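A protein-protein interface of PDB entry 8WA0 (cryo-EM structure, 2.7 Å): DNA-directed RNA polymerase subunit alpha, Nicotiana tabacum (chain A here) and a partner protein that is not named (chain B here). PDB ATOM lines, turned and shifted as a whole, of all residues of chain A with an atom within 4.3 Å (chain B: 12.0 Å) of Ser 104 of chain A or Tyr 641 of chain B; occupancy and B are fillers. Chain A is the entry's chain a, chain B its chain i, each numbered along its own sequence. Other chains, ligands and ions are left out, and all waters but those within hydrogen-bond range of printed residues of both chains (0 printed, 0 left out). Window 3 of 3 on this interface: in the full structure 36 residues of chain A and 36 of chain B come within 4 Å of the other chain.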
ATOM      1  N   SER A  98      14.493 -19.340  -1.674  1.00  0.00           N
ATOM      2  CA  SER A  98      14.230 -20.695  -2.128  1.00  0.00           C
ATOM      3  C   SER A  98      13.525 -21.505  -1.063  1.00  0.00           C
ATOM      4  O   SER A  98      13.718 -21.242   0.092  1.00  0.00           O
ATOM      5  CB  SER A  98      15.535 -21.384  -2.439  1.00  0.00           C
ATOM      6  OG  SER A  98      15.342 -22.741  -2.769  1.00  0.00           O
ATOM      7  N   LEU A 100      13.620 -25.118  -1.056  1.00  0.00           N
ATOM      8  CA  LEU A 100      14.077 -26.503  -1.098  1.00  0.00           C
ATOM      9  C   LEU A 100      15.477 -26.746  -0.665  1.00  0.00           C
ATOM     10  O   LEU A 100      16.310 -25.881  -0.746  1.00  0.00           O
ATOM     11  CB  LEU A 100      13.884 -27.073  -2.478  1.00  0.00           C
ATOM     12  CG  LEU A 100      12.514 -26.953  -3.146  1.00  0.00           C
ATOM     13  CD1 LEU A 100      12.611 -27.158  -4.644  1.00  0.00           C
ATOM     14  CD2 LEU A 100      11.513 -27.912  -2.534  1.00  0.00           C
ATOM     15  N   TYR A 101      15.761 -27.940  -0.226  1.00  0.00           N
ATOM     16  CA  TYR A 101      17.031 -28.243   0.352  1.00  0.00           C
ATOM     17  C   TYR A 101      18.001 -28.897  -0.557  1.00  0.00           C
ATOM     18  O   TYR A 101      17.633 -29.412  -1.567  1.00  0.00           O
ATOM     19  CB  TYR A 101      16.830 -29.096   1.580  1.00  0.00           C
ATOM     20  CG  TYR A 101      16.126 -28.424   2.721  1.00  0.00           C
ATOM     21  CD1 TYR A 101      16.809 -27.610   3.600  1.00  0.00           C
ATOM     22  CD2 TYR A 101      14.784 -28.623   2.931  1.00  0.00           C
ATOM     23  CE1 TYR A 101      16.156 -27.000   4.647  1.00  0.00           C
ATOM     24  CE2 TYR A 101      14.124 -28.018   3.965  1.00  0.00           C
ATOM     25  CZ  TYR A 101      14.811 -27.213   4.818  1.00  0.00           C
ATOM     26  OH  TYR A 101      14.139 -26.623   5.848  1.00  0.00           O
ATOM     27  N   GLY A 102      19.275 -28.837  -0.224  1.00  0.00           N
ATOM     28  CA  GLY A 102      20.285 -29.359  -1.105  1.00  0.00           C
ATOM     29  C   GLY A 102      21.154 -28.276  -1.697  1.00  0.00           C
ATOM     30  O   GLY A 102      20.916 -27.119  -1.403  1.00  0.00           O
ATOM     31  N   THR A 103      22.146 -28.631  -2.506  1.00  0.00           N
ATOM     32  CA  THR A 103      23.056 -27.650  -3.066  1.00  0.00           C
ATOM     33  C   THR A 103      22.723 -27.405  -4.508  1.00  0.00           C
ATOM     34  O   THR A 103      22.311 -28.314  -5.203  1.00  0.00           O
ATOM     35  CB  THR A 103      24.496 -28.141  -2.972  1.00  0.00           C
ATOM     36  OG1 THR A 103      24.706 -28.747  -1.691  1.00  0.00           O
ATOM     37  CG2 THR A 103      25.476 -26.996  -3.148  1.00  0.00           C
ATOM     38  N   SER A 104      22.894 -26.181  -4.971  1.00  0.00           N
ATOM     39  CA  SER A 104      22.579 -25.835  -6.341  1.00  0.00           C
ATOM     40  C   SER A 104      23.698 -25.005  -6.912  1.00  0.00           C
ATOM     41  O   SER A 104      24.472 -24.441  -6.167  1.00  0.00           O
ATOM     42  CB  SER A 104      21.279 -25.066  -6.396  1.00  0.00           C
ATOM     43  OG  SER A 104      21.336 -23.934  -5.555  1.00  0.00           O
ATOM     44  N   ASP A 105      23.807 -24.932  -8.226  1.00  0.00           N
ATOM     45  CA  ASP A 105      24.919 -24.231  -8.834  1.00  0.00           C
ATOM     46  C   ASP A 105      24.515 -23.101  -9.741  1.00  0.00           C
ATOM     47  O   ASP A 105      23.548 -23.213 -10.472  1.00  0.00           O
ATOM     48  CB  ASP A 105      25.756 -25.213  -9.621  1.00  0.00           C
ATOM     49  CG  ASP A 105      26.273 -26.349  -8.772  1.00  0.00           C
ATOM     50  OD1 ASP A 105      25.565 -27.368  -8.642  1.00  0.00           O
ATOM     51  OD2 ASP A 105      27.389 -26.224  -8.232  1.00  0.00           O
ATOM     52  N   PRO A 124      19.412 -21.245 -11.046  1.00  0.00           N
ATOM     53  CA  PRO A 124      18.585 -22.390 -11.396  1.00  0.00           C
ATOM     54  C   PRO A 124      17.113 -22.061 -11.287  1.00  0.00           C
ATOM     55  O   PRO A 124      16.755 -20.962 -10.916  1.00  0.00           O
ATOM     56  CB  PRO A 124      18.940 -23.393 -10.305  1.00  0.00           C
ATOM     57  CG  PRO A 124      20.272 -23.026  -9.832  1.00  0.00           C
ATOM     58  CD  PRO A 124      20.128 -21.555  -9.777  1.00  0.00           C
ATOM     59  N   TYR A 126      14.560 -23.037  -9.167  1.00  0.00           N
ATOM     60  CA  TYR A 126      14.086 -22.791  -7.794  1.00  0.00           C
ATOM     61  C   TYR A 126      14.556 -21.553  -7.014  1.00  0.00           C
ATOM     62  O   TYR A 126      13.786 -20.999  -6.268  1.00  0.00           O
ATOM     63  CB  TYR A 126      14.327 -24.048  -6.995  1.00  0.00           C
ATOM     64  CG  TYR A 126      13.656 -25.225  -7.634  1.00  0.00           C
ATOM     65  CD1 TYR A 126      12.281 -25.236  -7.821  1.00  0.00           C
ATOM     66  CD2 TYR A 126      14.387 -26.312  -8.075  1.00  0.00           C
ATOM     67  CE1 TYR A 126      11.649 -26.308  -8.418  1.00  0.00           C
ATOM     68  CE2 TYR A 126      13.765 -27.390  -8.671  1.00  0.00           C
ATOM     69  CZ  TYR A 126      12.398 -27.380  -8.838  1.00  0.00           C
ATOM     70  OH  TYR A 126      11.778 -28.450  -9.427  1.00  0.00           O
ATOM     71  N   VAL A 127      15.812 -21.157  -7.135  1.00  0.00           N
ATOM     72  CA  VAL A 127      16.325 -19.978  -6.477  1.00  0.00           C
ATOM     73  C   VAL A 127      16.058 -18.680  -7.212  1.00  0.00           C
ATOM     74  O   VAL A 127      16.125 -18.655  -8.414  1.00  0.00           O
ATOM     75  CB  VAL A 127      17.808 -20.134  -6.225  1.00  0.00           C
ATOM     76  CG1 VAL A 127      18.251 -19.225  -5.099  1.00  0.00           C
ATOM     77  CG2 VAL A 127      18.122 -21.577  -5.891  1.00  0.00           C
ATOM     78  N   LEU A 149      29.285 -20.344  -8.603  1.00  0.00           N
ATOM     79  CA  LEU A 149      28.763 -20.218  -7.250  1.00  0.00           C
ATOM     80  C   LEU A 149      27.925 -21.389  -6.768  1.00  0.00           C
ATOM     81  O   LEU A 149      27.273 -22.031  -7.564  1.00  0.00           O
ATOM     82  CB  LEU A 149      27.903 -18.969  -7.211  1.00  0.00           C
ATOM     83  CG  LEU A 149      28.462 -17.646  -7.713  1.00  0.00           C
ATOM     84  CD1 LEU A 149      27.329 -16.727  -8.118  1.00  0.00           C
ATOM     85  CD2 LEU A 149      29.318 -17.005  -6.639  1.00  0.00           C
ATOM     86  N   GLN A 150      27.937 -21.677  -5.472  1.00  0.00           N
ATOM     87  CA  GLN A 150      27.091 -22.731  -4.908  1.00  0.00           C
ATOM     88  C   GLN A 150      26.138 -22.186  -3.863  1.00  0.00           C
ATOM     89  O   GLN A 150      26.561 -21.453  -2.996  1.00  0.00           O
ATOM     90  CB  GLN A 150      27.929 -23.817  -4.278  1.00  0.00           C
ATOM     91  CG  GLN A 150      28.591 -24.737  -5.274  1.00  0.00           C
ATOM     92  CD  GLN A 150      29.192 -25.945  -4.601  1.00  0.00           C
ATOM     93  OE1 GLN A 150      29.097 -26.099  -3.385  1.00  0.00           O
ATOM     94  NE2 GLN A 150      29.812 -26.814  -5.387  1.00  0.00           N
ATOM     95  N   ILE A 151      24.863 -22.550  -3.909  1.00  0.00           N
ATOM     96  CA  ILE A 151      23.866 -21.991  -3.007  1.00  0.00           C
ATOM     97  C   ILE A 151      23.214 -23.066  -2.159  1.00  0.00           C
ATOM     98  O   ILE A 151      23.012 -24.163  -2.635  1.00  0.00           O
ATOM     99  CB  ILE A 151      22.792 -21.266  -3.829  1.00  0.00           C
ATOM    100  CG1 ILE A 151      23.440 -20.248  -4.761  1.00  0.00           C
ATOM    101  CG2 ILE A 151      21.773 -20.582  -2.939  1.00  0.00           C
ATOM    102  CD1 ILE A 151      22.472 -19.596  -5.716  1.00  0.00           C
ATOM    103  N   ARG B 308       3.107 -19.217  -3.418  1.00  0.00           N
ATOM    104  CA  ARG B 308       4.530 -19.088  -3.196  1.00  0.00           C
ATOM    105  C   ARG B 308       5.212 -20.395  -2.886  1.00  0.00           C
ATOM    106  O   ARG B 308       6.343 -20.617  -3.287  1.00  0.00           O
ATOM    107  CB  ARG B 308       4.843 -18.007  -2.178  1.00  0.00           C
ATOM    108  CG  ARG B 308       4.587 -16.630  -2.769  1.00  0.00           C
ATOM    109  CD  ARG B 308       5.036 -15.483  -1.888  1.00  0.00           C
ATOM    110  NE  ARG B 308       6.446 -15.555  -1.521  1.00  0.00           N
ATOM    111  CZ  ARG B 308       7.126 -14.542  -0.993  1.00  0.00           C
ATOM    112  NH1 ARG B 308       6.529 -13.377  -0.792  1.00  0.00           N
ATOM    113  NH2 ARG B 308       8.400 -14.683  -0.674  1.00  0.00           N
ATOM    114  N   LYS B 310       4.271 -23.357  -3.911  1.00  0.00           N
ATOM    115  CA  LYS B 310       3.773 -24.357  -4.831  1.00  0.00           C
ATOM    116  C   LYS B 310       4.693 -25.495  -5.034  1.00  0.00           C
ATOM    117  O   LYS B 310       4.265 -26.625  -5.141  1.00  0.00           O
ATOM    118  CB  LYS B 310       3.591 -23.729  -6.191  1.00  0.00           C
ATOM    119  N   ASP B 311       5.956 -25.224  -5.089  1.00  0.00           N
ATOM    120  CA  ASP B 311       6.911 -26.257  -5.250  1.00  0.00           C
ATOM    121  C   ASP B 311       6.992 -27.278  -4.182  1.00  0.00           C
ATOM    122  O   ASP B 311       7.175 -28.443  -4.473  1.00  0.00           O
ATOM    123  CB  ASP B 311       8.280 -25.639  -5.449  1.00  0.00           C
ATOM    124  CG  ASP B 311       8.714 -24.734  -4.295  1.00  0.00           C
ATOM    125  OD1 ASP B 311       7.858 -24.220  -3.543  1.00  0.00           O
ATOM    126  OD2 ASP B 311       9.936 -24.527  -4.150  1.00  0.00           O
ATOM    127  N   ALA B 312       6.880 -26.888  -2.939  1.00  0.00           N
ATOM    128  CA  ALA B 312       7.081 -27.826  -1.868  1.00  0.00           C
ATOM    129  C   ALA B 312       5.931 -28.274  -0.956  1.00  0.00           C
ATOM    130  O   ALA B 312       6.171 -28.953   0.023  1.00  0.00           O
ATOM    131  CB  ALA B 312       8.198 -27.300  -1.029  1.00  0.00           C
ATOM    132  N   PRO B 618       7.882 -41.429  -1.236  1.00  0.00           N
ATOM    133  CA  PRO B 618       9.115 -40.942  -1.868  1.00  0.00           C
ATOM    134  C   PRO B 618       8.837 -40.215  -3.166  1.00  0.00           C
ATOM    135  O   PRO B 618       8.200 -40.805  -4.027  1.00  0.00           O
ATOM    136  CB  PRO B 618       9.885 -42.215  -2.127  1.00  0.00           C
ATOM    137  CG  PRO B 618       9.429 -43.151  -1.066  1.00  0.00           C
ATOM    138  CD  PRO B 618       7.970 -42.855  -0.887  1.00  0.00           C
ATOM    139  N   LYS B 619       9.300 -38.976  -3.325  1.00  0.00           N
ATOM    140  CA  LYS B 619       8.961 -38.187  -4.517  1.00  0.00           C
ATOM    141  C   LYS B 619       9.506 -38.716  -5.817  1.00  0.00           C
ATOM    142  O   LYS B 619       8.765 -38.843  -6.787  1.00  0.00           O
ATOM    143  CB  LYS B 619       9.503 -36.776  -4.314  1.00  0.00           C
ATOM    144  CG  LYS B 619       9.010 -35.736  -5.300  1.00  0.00           C
ATOM    145  CD  LYS B 619       9.576 -34.373  -4.941  1.00  0.00           C
ATOM    146  CE  LYS B 619       8.994 -33.280  -5.817  1.00  0.00           C
ATOM    147  NZ  LYS B 619       9.563 -31.947  -5.477  1.00  0.00           N
ATOM    148  N   GLU B 620      10.786 -39.040  -5.841  1.00  0.00           N
ATOM    149  CA  GLU B 620      11.434 -39.605  -7.018  1.00  0.00           C
ATOM    150  C   GLU B 620      12.766 -39.960  -6.411  1.00  0.00           C
ATOM    151  O   GLU B 620      13.014 -39.608  -5.258  1.00  0.00           O
ATOM    152  CB  GLU B 620      11.613 -38.613  -8.157  1.00  0.00           C
ATOM    153  CG  GLU B 620      10.752 -38.915  -9.371  1.00  0.00           C
ATOM    154  CD  GLU B 620      10.838 -40.365  -9.802  1.00  0.00           C
ATOM    155  OE1 GLU B 620      11.960 -40.914  -9.855  1.00  0.00           O
ATOM    156  OE2 GLU B 620       9.780 -40.954 -10.105  1.00  0.00           O
ATOM    157  N   GLY B 621      13.652 -40.617  -7.144  1.00  0.00           N
ATOM    158  CA  GLY B 621      14.883 -41.032  -6.501  1.00  0.00           C
ATOM    159  C   GLY B 621      14.506 -41.873  -5.309  1.00  0.00           C
ATOM    160  O   GLY B 621      14.968 -41.630  -4.200  1.00  0.00           O
ATOM    161  N   MET B 622      13.630 -42.844  -5.530  1.00  0.00           N
ATOM    162  CA  MET B 622      13.171 -43.704  -4.454  1.00  0.00           C
ATOM    163  C   MET B 622      14.121 -44.850  -4.168  1.00  0.00           C
ATOM    164  O   MET B 622      13.818 -45.997  -4.472  1.00  0.00           O
ATOM    165  CB  MET B 622      11.821 -44.275  -4.851  1.00  0.00           C
ATOM    166  N   ILE B 633       9.102 -41.364   3.810  1.00  0.00           N
ATOM    167  CA  ILE B 633      10.165 -40.408   4.100  1.00  0.00           C
ATOM    168  C   ILE B 633       9.685 -39.192   4.863  1.00  0.00           C
ATOM    169  O   ILE B 633       8.513 -38.879   4.827  1.00  0.00           O
ATOM    170  CB  ILE B 633      10.806 -39.891   2.812  1.00  0.00           C
ATOM    171  CG1 ILE B 633       9.772 -39.227   1.911  1.00  0.00           C
ATOM    172  CG2 ILE B 633      11.513 -41.007   2.063  1.00  0.00           C
ATOM    173  CD1 ILE B 633      10.363 -38.622   0.661  1.00  0.00           C
ATOM    174  N   LYS B 634      10.564 -38.505   5.568  1.00  0.00           N
ATOM    175  CA  LYS B 634      10.234 -37.286   6.309  1.00  0.00           C
ATOM    176  C   LYS B 634      10.085 -36.095   5.418  1.00  0.00           C
ATOM    177  O   LYS B 634      10.447 -36.149   4.251  1.00  0.00           O
ATOM    178  CB  LYS B 634      11.263 -37.032   7.367  1.00  0.00           C
ATOM    179  CG  LYS B 634      11.279 -38.070   8.464  1.00  0.00           C
ATOM    180  CD  LYS B 634      12.483 -37.867   9.362  1.00  0.00           C
ATOM    181  CE  LYS B 634      13.771 -37.934   8.558  1.00  0.00           C
ATOM    182  NZ  LYS B 634      14.970 -37.680   9.401  1.00  0.00           N
ATOM    183  N   SER B 635       9.516 -35.023   5.921  1.00  0.00           N
ATOM    184  CA  SER B 635       9.260 -33.847   5.106  1.00  0.00           C
ATOM    185  C   SER B 635      10.488 -33.187   4.546  1.00  0.00           C
ATOM    186  O   SER B 635      10.448 -32.662   3.449  1.00  0.00           O
ATOM    187  CB  SER B 635       8.440 -32.825   5.858  1.00  0.00           C
ATOM    188  OG  SER B 635       7.998 -31.789   5.006  1.00  0.00           O
ATOM    189  N   VAL B 636      11.572 -33.177   5.290  1.00  0.00           N
ATOM    190  CA  VAL B 636      12.774 -32.594   4.808  1.00  0.00           C
ATOM    191  C   VAL B 636      13.173 -33.342   3.599  1.00  0.00           C
ATOM    192  O   VAL B 636      13.562 -32.752   2.600  1.00  0.00           O
ATOM    193  CB  VAL B 636      13.899 -32.744   5.809  1.00  0.00           C
ATOM    194  CG1 VAL B 636      15.090 -31.889   5.413  1.00  0.00           C
ATOM    195  CG2 VAL B 636      13.418 -32.360   7.196  1.00  0.00           C
ATOM    196  N   THR B 637      13.069 -34.642   3.657  1.00  0.00           N
ATOM    197  CA  THR B 637      13.438 -35.456   2.550  1.00  0.00           C
ATOM    198  C   THR B 637      12.563 -35.180   1.387  1.00  0.00           C
ATOM    199  O   THR B 637      13.052 -35.181   0.276  1.00  0.00           O
ATOM    200  CB  THR B 637      13.432 -36.905   2.941  1.00  0.00           C
ATOM    201  OG1 THR B 637      13.909 -37.041   4.284  1.00  0.00           O
ATOM    202  CG2 THR B 637      14.321 -37.712   2.009  1.00  0.00           C
ATOM    203  N   GLU B 638      11.283 -34.947   1.563  1.00  0.00           N
ATOM    204  CA  GLU B 638      10.468 -34.748   0.408  1.00  0.00           C
ATOM    205  C   GLU B 638      10.933 -33.545  -0.289  1.00  0.00           C
ATOM    206  O   GLU B 638      10.958 -33.498  -1.501  1.00  0.00           O
ATOM    207  CB  GLU B 638       8.996 -34.581   0.706  1.00  0.00           C
ATOM    208  CG  GLU B 638       8.109 -35.311  -0.281  1.00  0.00           C
ATOM    209  CD  GLU B 638       7.019 -34.438  -0.829  1.00  0.00           C
ATOM    210  OE1 GLU B 638       6.925 -33.281  -0.398  1.00  0.00           O
ATOM    211  OE2 GLU B 638       6.256 -34.902  -1.686  1.00  0.00           O
ATOM    212  N   ARG B 639      11.288 -32.538   0.463  1.00  0.00           N
ATOM    213  CA  ARG B 639      11.684 -31.304  -0.119  1.00  0.00           C
ATOM    214  C   ARG B 639      13.136 -31.294  -0.438  1.00  0.00           C
ATOM    215  O   ARG B 639      13.902 -30.611   0.217  1.00  0.00           O
ATOM    216  CB  ARG B 639      11.337 -30.201   0.830  1.00  0.00           C
ATOM    217  CG  ARG B 639       9.890 -30.103   1.240  1.00  0.00           C
ATOM    218  CD  ARG B 639       9.731 -28.889   2.124  1.00  0.00           C
ATOM    219  NE  ARG B 639       8.373 -28.713   2.600  1.00  0.00           N
ATOM    220  CZ  ARG B 639       7.963 -27.649   3.271  1.00  0.00           C
ATOM    221  NH1 ARG B 639       8.809 -26.666   3.528  1.00  0.00           N
ATOM    222  NH2 ARG B 639       6.707 -27.558   3.674  1.00  0.00           N
ATOM    223  N   GLU B 640      13.543 -32.040  -1.445  1.00  0.00           N
ATOM    224  CA  GLU B 640      14.931 -32.090  -1.868  1.00  0.00           C
ATOM    225  C   GLU B 640      14.974 -31.540  -3.249  1.00  0.00           C
ATOM    226  O   GLU B 640      13.967 -31.502  -3.921  1.00  0.00           O
ATOM    227  CB  GLU B 640      15.561 -33.446  -1.747  1.00  0.00           C
ATOM    228  CG  GLU B 640      15.960 -33.811  -0.334  1.00  0.00           C
ATOM    229  CD  GLU B 640      17.028 -32.901   0.231  1.00  0.00           C
ATOM    230  OE1 GLU B 640      17.913 -32.461  -0.535  1.00  0.00           O
ATOM    231  OE2 GLU B 640      16.994 -32.635   1.450  1.00  0.00           O
ATOM    232  N   TYR B 641      16.134 -31.095  -3.686  1.00  0.00           N
ATOM    233  CA  TYR B 641      16.207 -30.388  -4.934  1.00  0.00           C
ATOM    234  C   TYR B 641      15.783 -31.082  -6.197  1.00  0.00           C
ATOM    235  O   TYR B 641      15.124 -30.458  -7.025  1.00  0.00           O
ATOM    236  CB  TYR B 641      17.557 -29.725  -5.108  1.00  0.00           C
ATOM    237  CG  TYR B 641      17.565 -28.260  -4.767  1.00  0.00           C
ATOM    238  CD1 TYR B 641      16.516 -27.436  -5.141  1.00  0.00           C
ATOM    239  CD2 TYR B 641      18.624 -27.697  -4.073  1.00  0.00           C
ATOM    240  CE1 TYR B 641      16.520 -26.091  -4.827  1.00  0.00           C
ATOM    241  CE2 TYR B 641      18.636 -26.355  -3.754  1.00  0.00           C
ATOM    242  CZ  TYR B 641      17.583 -25.557  -4.134  1.00  0.00           C
ATOM    243  OH  TYR B 641      17.594 -24.220  -3.818  1.00  0.00           O
ATOM    244  N   ARG B 642      16.107 -32.336  -6.393  1.00  0.00           N
ATOM    245  CA  ARG B 642      15.614 -32.946  -7.608  1.00  0.00           C
ATOM    246  C   ARG B 642      15.128 -34.349  -7.369  1.00  0.00           C
ATOM    247  O   ARG B 642      14.878 -34.738  -6.232  1.00  0.00           O
ATOM    248  CB  ARG B 642      16.689 -32.935  -8.688  1.00  0.00           C
ATOM    249  CG  ARG B 642      17.925 -33.749  -8.354  1.00  0.00           C
ATOM    250  CD  ARG B 642      18.873 -33.793  -9.539  1.00  0.00           C
ATOM    251  NE  ARG B 642      20.176 -34.338  -9.175  1.00  0.00           N
ATOM    252  CZ  ARG B 642      21.211 -33.601  -8.779  1.00  0.00           C
ATOM    253  NH1 ARG B 642      22.359 -34.182  -8.467  1.00  0.00           N
ATOM    254  NH2 ARG B 642      21.098 -32.281  -8.700  1.00  0.00           N
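The guanidinium group of Arg 639 of chain B sits at hydrogen-bond distance from the backbone carbonyl oxygen of Ala 312 of chain B (3.4 Å). O of Ser 104 of chain A is in hydrogen-bond range of N of Ile 151 of chain A (3.0 Å). The side-chain hydroxyl (OG) of Ser 98 of chain A sits at hydrogen-bond distance from the backbone NH (N) of Leu 100 of chain A (3.4 Å).
Ser 104 of chain A touches just one residue of chain B: Tyr 641. Of chain A, only Ser 98, Leu 100, Tyr 101, Gly 102, Thr 103, Ser 104, Tyr 126 and Val 127 come within 4 Å of Tyr 641 of chain B. Ser 98 of chain A touches one residue of chain B. Of chain B, only Asp 311 (3.7 Å), Ala 312 (3.7 Å) and Tyr 641 (3.6 Å) come within 4 Å of Leu 100 of chain A. Gly 102 of chain A touches just these residues of chain B: Glu 640 (3.9 Å) and Tyr 641 (3.4 Å). Thr 103 of chain A touches just one residue of chain B: Tyr 641 (3.9 Å). No residue of chain B comes within 4 Å of Asp 105 of chain A. No residue of chain B comes within 4 Å of Pro 124 of chain A. Of chain B, only Tyr 641 comes within 4 Å of Tyr 126 of chain A. No residue of chain B comes within 4 Å of Ile 151 of chain A. Printed residues of chain A within 4 Å of Asp 311 of chain B: Leu 100. Printed residues of chain A within 4 Å of Glu 640 of chain B: Tyr 101 (3.2 Å) and Gly 102 (3.9 Å). Met 622 of chain B touches none of the printed residues of chain A. The nearest residue of chain B that does not touch Ser 104 of chain A is Arg 642 of chain B (7.0 Å). The nearest printed residue of chain A that does not touch Tyr 641 of chain B is Ile 151 of chain A (5.0 Å).
Printed residues of chain A that touch a printed residue of chain B: Ser 98, Leu 100, Tyr 101, Gly 102, Thr 103, Ser 104, Tyr 126 and Val 127. Hydrophobic or aromatic side chains of chain B that line the printed part of chain A: Ala 312 and Tyr 641. Among the printed residues, no Asp or Glu carboxylate lies within 4 Å of a Lys or Arg side-chain nitrogen of the other chain.
The backbone NH of Tyr 641 of chain B lies within hydrogen-bond range of the backbone carbonyl oxygen of Tyr 101 of chain A (3.1 Å). The backbone NH (N) of Tyr 101 of chain A is in hydrogen-bond range of the backbone carbonyl oxygen (O) of Arg 639 of chain B (3.3 Å). The side-chain hydroxyl of Tyr 641 of chain B is in hydrogen-bond range of the side-chain hydroxyl of Ser 98 of chain A (2.9 Å). The side-chain carboxylate (OE1) of Glu 640 of chain B sits close to the backbone carbonyl oxygen (O) of Tyr 101 of chain A (3.2 Å).
Among the printed residues, merely in contact across the chains: Leu 100 of chain A with Asp 311 of chain B, Leu 100 of chain A with Ala 312 of chain B, Leu 100 of chain A with Tyr 641 of chain B, Gly 102 of chain A with Glu 640 of chain B, Gly 102 of chain A with Tyr 641 of chain B, Thr 103 of chain A with Tyr 641 of chain B, Ser 104 of chain A with Tyr 641 of chain B, Tyr 126 of chain A with Tyr 641 of chain B and Val 127 of chain A with Tyr 641 of chain B.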
